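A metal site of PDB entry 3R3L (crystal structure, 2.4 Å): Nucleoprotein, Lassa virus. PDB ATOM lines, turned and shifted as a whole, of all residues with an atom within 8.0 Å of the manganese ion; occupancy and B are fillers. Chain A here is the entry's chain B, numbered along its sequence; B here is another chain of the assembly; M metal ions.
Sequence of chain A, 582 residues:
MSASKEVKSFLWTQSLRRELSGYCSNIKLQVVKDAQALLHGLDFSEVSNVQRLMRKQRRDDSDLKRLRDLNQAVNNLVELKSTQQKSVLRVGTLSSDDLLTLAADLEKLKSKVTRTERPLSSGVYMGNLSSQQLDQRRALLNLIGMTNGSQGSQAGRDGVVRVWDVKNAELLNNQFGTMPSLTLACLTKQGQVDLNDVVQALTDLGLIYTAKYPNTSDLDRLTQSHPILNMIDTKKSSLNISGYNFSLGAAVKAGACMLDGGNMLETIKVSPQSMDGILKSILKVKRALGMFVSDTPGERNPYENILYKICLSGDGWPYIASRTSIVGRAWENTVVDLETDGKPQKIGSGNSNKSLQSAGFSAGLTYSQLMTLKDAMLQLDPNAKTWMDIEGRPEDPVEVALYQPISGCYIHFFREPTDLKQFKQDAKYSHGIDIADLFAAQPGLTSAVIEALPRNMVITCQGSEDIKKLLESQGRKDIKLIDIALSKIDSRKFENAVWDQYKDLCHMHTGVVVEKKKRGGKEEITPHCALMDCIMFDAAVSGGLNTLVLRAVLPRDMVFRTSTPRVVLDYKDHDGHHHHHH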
ATOM      1  N   GLN A 200      -4.784  -6.417   3.888  1.00  0.00           N
ATOM      2  CA  GLN A 200      -3.422  -6.952   4.000  1.00  0.00           C
ATOM      3  C   GLN A 200      -3.287  -7.834   5.244  1.00  0.00           C
ATOM      4  O   GLN A 200      -2.288  -8.546   5.408  1.00  0.00           O
ATOM      5  CB  GLN A 200      -2.382  -5.828   4.040  1.00  0.00           C
ATOM      6  CG  GLN A 200      -2.657  -4.617   3.138  1.00  0.00           C
ATOM      7  CD  GLN A 200      -2.148  -4.758   1.712  1.00  0.00           C
ATOM      8  OE1 GLN A 200      -2.630  -5.591   0.943  1.00  0.00           O
ATOM      9  NE2 GLN A 200      -1.185  -3.921   1.344  1.00  0.00           N
ATOM     10  N   ALA A 201      -4.279  -7.780   6.136  1.00  0.00           N
ATOM     11  CA  ALA A 201      -4.292  -8.607   7.333  1.00  0.00           C
ATOM     12  C   ALA A 201      -4.895  -9.977   7.033  1.00  0.00           C
ATOM     13  O   ALA A 201      -4.351 -11.012   7.435  1.00  0.00           O
ATOM     14  CB  ALA A 201      -5.065  -7.932   8.447  1.00  0.00           C
ATOM     15  N   LEU A 202      -6.022  -9.972   6.335  1.00  0.00           N
ATOM     16  CA  LEU A 202      -6.711 -11.211   5.978  1.00  0.00           C
ATOM     17  C   LEU A 202      -6.037 -11.904   4.795  1.00  0.00           C
ATOM     18  O   LEU A 202      -6.290 -13.082   4.535  1.00  0.00           O
ATOM     19  CB  LEU A 202      -8.197 -10.938   5.726  1.00  0.00           C
ATOM     20  CG  LEU A 202      -8.985 -10.212   6.840  1.00  0.00           C
ATOM     21  CD1 LEU A 202     -10.371  -9.811   6.372  1.00  0.00           C
ATOM     22  CD2 LEU A 202      -9.071 -11.029   8.122  1.00  0.00           C
ATOM     23  N   THR A 203      -5.176 -11.177   4.095  1.00  0.00           N
ATOM     24  CA  THR A 203      -4.313 -11.774   3.060  1.00  0.00           C
ATOM     25  C   THR A 203      -3.304 -12.731   3.701  1.00  0.00           C
ATOM     26  O   THR A 203      -3.070 -13.839   3.189  1.00  0.00           O
ATOM     27  CB  THR A 203      -3.615 -10.691   2.200  1.00  0.00           C
ATOM     28  OG1 THR A 203      -4.580 -10.064   1.347  1.00  0.00           O
ATOM     29  CG2 THR A 203      -2.504 -11.279   1.333  1.00  0.00           C
ATOM     30  N   ASP A 204      -2.722 -12.321   4.816  1.00  0.00           N
ATOM     31  CA  ASP A 204      -1.753 -13.160   5.535  1.00  0.00           C
ATOM     32  C   ASP A 204      -2.434 -14.315   6.261  1.00  0.00           C
ATOM     33  O   ASP A 204      -1.887 -15.419   6.349  1.00  0.00           O
ATOM     34  CB  ASP A 204      -0.902 -12.327   6.483  1.00  0.00           C
ATOM     35  CG  ASP A 204       0.080 -11.426   5.740  1.00  0.00           C
ATOM     36  OD1 ASP A 204       0.107 -11.471   4.492  1.00  0.00           O
ATOM     37  OD2 ASP A 204       0.823 -10.664   6.397  1.00  0.00           O
ATOM     38  N   LEU A 205      -3.641 -14.067   6.774  1.00  0.00           N
ATOM     39  CA  LEU A 205      -4.484 -15.126   7.318  1.00  0.00           C
ATOM     40  C   LEU A 205      -4.910 -16.081   6.206  1.00  0.00           C
ATOM     41  O   LEU A 205      -4.887 -17.302   6.389  1.00  0.00           O
ATOM     42  CB  LEU A 205      -5.713 -14.517   8.010  1.00  0.00           C
ATOM     43  CG  LEU A 205      -6.696 -15.465   8.698  1.00  0.00           C
ATOM     44  CD1 LEU A 205      -6.040 -16.220   9.857  1.00  0.00           C
ATOM     45  CD2 LEU A 205      -7.899 -14.683   9.188  1.00  0.00           C
ATOM     46  N   ARG A 221       0.381 -14.211  16.433  1.00  0.00           N
ATOM     47  CA  ARG A 221       1.629 -13.696  15.886  1.00  0.00           C
ATOM     48  C   ARG A 221       1.428 -12.704  14.734  1.00  0.00           C
ATOM     49  O   ARG A 221       2.239 -11.808  14.536  1.00  0.00           O
ATOM     50  CB  ARG A 221       2.529 -14.861  15.463  1.00  0.00           C
ATOM     51  CG  ARG A 221       3.040 -15.667  16.644  1.00  0.00           C
ATOM     52  CD  ARG A 221       4.047 -16.710  16.214  1.00  0.00           C
ATOM     53  NE  ARG A 221       3.416 -17.999  15.932  1.00  0.00           N
ATOM     54  CZ  ARG A 221       3.259 -18.985  16.825  1.00  0.00           C
ATOM     55  NH1 ARG A 221       3.666 -18.832  18.078  1.00  0.00           N
ATOM     56  NH2 ARG A 221       2.677 -20.120  16.450  1.00  0.00           N
ATOM     57  N   LEU A 222       0.337 -12.880  13.994  1.00  0.00           N
ATOM     58  CA  LEU A 222      -0.049 -11.922  12.947  1.00  0.00           C
ATOM     59  C   LEU A 222      -0.508 -10.625  13.596  1.00  0.00           C
ATOM     60  O   LEU A 222      -0.193  -9.529  13.102  1.00  0.00           O
ATOM     61  CB  LEU A 222      -1.175 -12.488  12.075  1.00  0.00           C
ATOM     62  CG  LEU A 222      -0.951 -13.666  11.133  1.00  0.00           C
ATOM     63  CD1 LEU A 222      -2.238 -13.956  10.388  1.00  0.00           C
ATOM     64  CD2 LEU A 222       0.179 -13.392  10.149  1.00  0.00           C
ATOM     65  N   THR A 223      -1.238 -10.757  14.691  1.00  0.00           N
ATOM     66  CA  THR A 223      -1.713  -9.631  15.503  1.00  0.00           C
ATOM     67  C   THR A 223      -0.609  -8.612  15.823  1.00  0.00           C
ATOM     68  O   THR A 223      -0.864  -7.401  15.889  1.00  0.00           O
ATOM     69  CB  THR A 223      -2.386 -10.143  16.802  1.00  0.00           C
ATOM     70  OG1 THR A 223      -3.713 -10.584  16.515  1.00  0.00           O
ATOM     71  CG2 THR A 223      -2.428  -9.089  17.878  1.00  0.00           C
ATOM     72  N   GLN A 224       0.616  -9.111  15.995  1.00  0.00           N
ATOM     73  CA  GLN A 224       1.781  -8.276  16.290  1.00  0.00           C
ATOM     74  C   GLN A 224       2.116  -7.346  15.131  1.00  0.00           C
ATOM     75  O   GLN A 224       2.581  -6.221  15.351  1.00  0.00           O
ATOM     76  CB  GLN A 224       2.980  -9.159  16.664  1.00  0.00           C
ATOM     77  CG  GLN A 224       2.797  -9.931  17.975  1.00  0.00           C
ATOM     78  CD  GLN A 224       3.525 -11.265  17.995  1.00  0.00           C
ATOM     79  OE1 GLN A 224       4.580 -11.424  17.384  1.00  0.00           O
ATOM     80  NE2 GLN A 224       2.949 -12.236  18.706  1.00  0.00           N
ATOM     81  N   SER A 225       1.876  -7.815  13.916  1.00  0.00           N
ATOM     82  CA  SER A 225       2.089  -7.022  12.697  1.00  0.00           C
ATOM     83  C   SER A 225       0.819  -6.336  12.202  1.00  0.00           C
ATOM     84  O   SER A 225       0.888  -5.245  11.612  1.00  0.00           O
ATOM     85  CB  SER A 225       2.652  -7.913  11.589  1.00  0.00           C
ATOM     86  OG  SER A 225       1.813  -9.029  11.376  1.00  0.00           O
ATOM     87  N   HIS A 226      -0.326  -6.968  12.429  1.00  0.00           N
ATOM     88  CA  HIS A 226      -1.644  -6.429  12.069  1.00  0.00           C
ATOM     89  C   HIS A 226      -2.571  -6.453  13.284  1.00  0.00           C
ATOM     90  O   HIS A 226      -3.201  -7.468  13.544  1.00  0.00           O
ATOM     91  CB  HIS A 226      -2.265  -7.226  10.925  1.00  0.00           C
ATOM     92  CG  HIS A 226      -1.373  -7.402   9.732  1.00  0.00           C
ATOM     93  ND1 HIS A 226      -1.267  -6.455   8.741  1.00  0.00           N
ATOM     94  CD2 HIS A 226      -0.542  -8.417   9.391  1.00  0.00           C
ATOM     95  CE1 HIS A 226      -0.408  -6.880   7.827  1.00  0.00           C
ATOM     96  NE2 HIS A 226       0.047  -8.067   8.197  1.00  0.00           N
ATOM     97  N   LEU A 229      -6.421  -8.010  14.049  1.00  0.00           N
ATOM     98  CA  LEU A 229      -6.734  -9.414  14.342  1.00  0.00           C
ATOM     99  C   LEU A 229      -6.920  -9.716  15.841  1.00  0.00           C
ATOM    100  O   LEU A 229      -7.177 -10.869  16.213  1.00  0.00           O
ATOM    101  CB  LEU A 229      -5.693 -10.324  13.710  1.00  0.00           C
ATOM    102  CG  LEU A 229      -5.537 -10.199  12.184  1.00  0.00           C
ATOM    103  CD1 LEU A 229      -4.099 -10.381  11.766  1.00  0.00           C
ATOM    104  CD2 LEU A 229      -6.445 -11.173  11.442  1.00  0.00           C
ATOM    105  N   VAL B 199      11.073  -7.329  10.515  1.00  0.00           N
ATOM    106  CA  VAL B 199      10.637  -8.282  11.533  1.00  0.00           C
ATOM    107  C   VAL B 199       9.165  -8.676  11.303  1.00  0.00           C
ATOM    108  O   VAL B 199       8.790  -9.829  11.530  1.00  0.00           O
ATOM    109  CB  VAL B 199      10.833  -7.704  12.958  1.00  0.00           C
ATOM    110  CG1 VAL B 199      10.214  -8.606  14.024  1.00  0.00           C
ATOM    111  CG2 VAL B 199      12.321  -7.497  13.255  1.00  0.00           C
ATOM    112  N   GLN B 200       8.356  -7.727  10.849  1.00  0.00           N
ATOM    113  CA  GLN B 200       6.945  -7.977  10.518  1.00  0.00           C
ATOM    114  C   GLN B 200       6.824  -9.015   9.399  1.00  0.00           C
ATOM    115  O   GLN B 200       6.085  -9.993   9.529  1.00  0.00           O
ATOM    116  CB  GLN B 200       6.250  -6.685  10.069  1.00  0.00           C
ATOM    117  CG  GLN B 200       6.345  -5.503  11.023  1.00  0.00           C
ATOM    118  CD  GLN B 200       5.378  -5.589  12.172  1.00  0.00           C
ATOM    119  OE1 GLN B 200       5.450  -6.498  13.005  1.00  0.00           O
ATOM    120  NE2 GLN B 200       4.474  -4.621  12.253  1.00  0.00           N
ATOM    121  N   ALA B 201       7.560  -8.775   8.320  1.00  0.00           N
ATOM    122  CA  ALA B 201       7.487  -9.568   7.102  1.00  0.00           C
ATOM    123  C   ALA B 201       7.906 -11.013   7.316  1.00  0.00           C
ATOM    124  O   ALA B 201       7.288 -11.934   6.797  1.00  0.00           O
ATOM    125  CB  ALA B 201       8.346  -8.934   6.014  1.00  0.00           C
ATOM    126  N   LEU B 202       8.977 -11.190   8.085  1.00  0.00           N
ATOM    127  CA  LEU B 202       9.557 -12.515   8.284  1.00  0.00           C
ATOM    128  C   LEU B 202       8.668 -13.393   9.156  1.00  0.00           C
ATOM    129  O   LEU B 202       8.607 -14.610   8.945  1.00  0.00           O
ATOM    130  CB  LEU B 202      10.972 -12.414   8.867  1.00  0.00           C
ATOM    131  CG  LEU B 202      12.092 -11.845   7.989  1.00  0.00           C
ATOM    132  CD1 LEU B 202      13.358 -11.698   8.804  1.00  0.00           C
ATOM    133  CD2 LEU B 202      12.359 -12.704   6.753  1.00  0.00           C
ATOM    134  N   THR B 203       7.982 -12.784  10.114  1.00  0.00           N
ATOM    135  CA  THR B 203       7.078 -13.502  11.021  1.00  0.00           C
ATOM    136  C   THR B 203       6.009 -14.271  10.257  1.00  0.00           C
ATOM    137  O   THR B 203       5.811 -15.467  10.466  1.00  0.00           O
ATOM    138  CB  THR B 203       6.398 -12.556  12.039  1.00  0.00           C
ATOM    139  OG1 THR B 203       7.334 -11.585  12.509  1.00  0.00           O
ATOM    140  CG2 THR B 203       5.860 -13.343  13.235  1.00  0.00           C
ATOM    141  N   ASP B 204       5.325 -13.571   9.347  1.00  0.00           N
ATOM    142  CA  ASP B 204       4.246 -14.157   8.569  1.00  0.00           C
ATOM    143  C   ASP B 204       4.737 -15.299   7.688  1.00  0.00           C
ATOM    144  O   ASP B 204       4.029 -16.297   7.494  1.00  0.00           O
ATOM    145  CB  ASP B 204       3.549 -13.089   7.725  1.00  0.00           C
ATOM    146  CG  ASP B 204       3.188 -11.861   8.531  1.00  0.00           C
ATOM    147  OD1 ASP B 204       3.110 -11.923   9.780  1.00  0.00           O
ATOM    148  OD2 ASP B 204       2.971 -10.796   7.916  1.00  0.00           O
ATOM    149  N   LEU B 205       5.960 -15.167   7.177  1.00  0.00           N
ATOM    150  CA  LEU B 205       6.629 -16.232   6.440  1.00  0.00           C
ATOM    151  C   LEU B 205       6.951 -17.399   7.377  1.00  0.00           C
ATOM    152  O   LEU B 205       6.732 -18.564   7.034  1.00  0.00           O
ATOM    153  CB  LEU B 205       7.900 -15.709   5.765  1.00  0.00           C
ATOM    154  CG  LEU B 205       8.680 -16.618   4.816  1.00  0.00           C
ATOM    155  CD1 LEU B 205       8.028 -16.703   3.451  1.00  0.00           C
ATOM    156  CD2 LEU B 205      10.118 -16.126   4.690  1.00  0.00           C
ATOM    157  N   LEU B 207       5.401 -18.274  10.094  1.00  0.00           N
ATOM    158  CA  LEU B 207       4.134 -18.941  10.380  1.00  0.00           C
ATOM    159  C   LEU B 207       3.722 -19.918   9.282  1.00  0.00           C
ATOM    160  O   LEU B 207       3.211 -20.995   9.580  1.00  0.00           O
ATOM    161  CB  LEU B 207       3.018 -17.904  10.585  1.00  0.00           C
ATOM    162  CG  LEU B 207       2.814 -17.405  12.005  1.00  0.00           C
ATOM    163  CD1 LEU B 207       2.075 -16.080  11.981  1.00  0.00           C
ATOM    164  CD2 LEU B 207       2.057 -18.440  12.831  1.00  0.00           C
ATOM    165  N   LEU B 222       2.824 -12.941  -0.603  1.00  0.00           N
ATOM    166  CA  LEU B 222       3.275 -12.288   0.625  1.00  0.00           C
ATOM    167  C   LEU B 222       3.896 -10.920   0.370  1.00  0.00           C
ATOM    168  O   LEU B 222       3.887 -10.056   1.249  1.00  0.00           O
ATOM    169  CB  LEU B 222       4.257 -13.181   1.396  1.00  0.00           C
ATOM    170  CG  LEU B 222       3.623 -14.120   2.425  1.00  0.00           C
ATOM    171  CD1 LEU B 222       4.693 -14.935   3.120  1.00  0.00           C
ATOM    172  CD2 LEU B 222       2.801 -13.334   3.450  1.00  0.00           C
ATOM    173  N   SER B 225       1.545  -7.466   0.588  1.00  0.00           N
ATOM    174  CA  SER B 225       1.489  -6.610   1.765  1.00  0.00           C
ATOM    175  C   SER B 225       2.873  -6.102   2.175  1.00  0.00           C
ATOM    176  O   SER B 225       3.038  -4.920   2.494  1.00  0.00           O
ATOM    177  CB  SER B 225       0.790  -7.312   2.934  1.00  0.00           C
ATOM    178  OG  SER B 225       1.283  -8.619   3.112  1.00  0.00           O
ATOM    179  N   HIS B 226       3.860  -7.001   2.160  1.00  0.00           N
ATOM    180  CA  HIS B 226       5.236  -6.683   2.568  1.00  0.00           C
ATOM    181  C   HIS B 226       6.155  -6.639   1.352  1.00  0.00           C
ATOM    182  O   HIS B 226       6.770  -7.647   1.008  1.00  0.00           O
ATOM    183  CB  HIS B 226       5.774  -7.729   3.558  1.00  0.00           C
ATOM    184  CG  HIS B 226       4.774  -8.176   4.577  1.00  0.00           C
ATOM    185  ND1 HIS B 226       4.563  -7.510   5.766  1.00  0.00           N
ATOM    186  CD2 HIS B 226       3.951  -9.251   4.597  1.00  0.00           C
ATOM    187  CE1 HIS B 226       3.638  -8.141   6.465  1.00  0.00           C
ATOM    188  NE2 HIS B 226       3.247  -9.199   5.782  1.00  0.00           N
HETATM  189 MN    MN M   1       1.677  -9.728   8.303  1.00  0.00          MN
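The manganese ion is bound by OD2 of Asp 204 of chain B, 1.7 Å away.
OD2 of Asp 204 of chain A binds the manganese ion (2.3 Å).
The manganese ion is bound by NE2 of His 226 of chain A, at 2.3 Å.
The manganese ion has three donor atoms within binding distance.
A ring nitrogen (NE2) of His 226 of chain B lies close to the side-chain carboxylate (OD2) of Asp 204 of chain B (2.7 Å).
OD2 of Asp 204 of chain A sits close to NE2 of His 226 of chain B (2.9 Å).
The side-chain carboxylate (OD1) of Asp 204 of chain A lies within hydrogen-bond range of the side-chain hydroxyl (OG) of Ser 225 of chain B (3.4 Å).
A ring nitrogen (NE2) of His 226 of chain B lies close to the side-chain hydroxyl (OG) of Ser 225 of chain B, 3.4 Å away.
The backbone carbonyl oxygen of Leu 222 of chain A lies within hydrogen-bond range of the side-chain hydroxyl of Ser 225 of chain A (2.7 Å).
OG of Ser 225 of chain A touches the manganese ion, at 3.2 Å.
His 226 of chain B touches the manganese ion (NE2 to MN, 3.0 Å).
Of the 24 residues printed, 5 come within 4 Å of the manganese ion.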
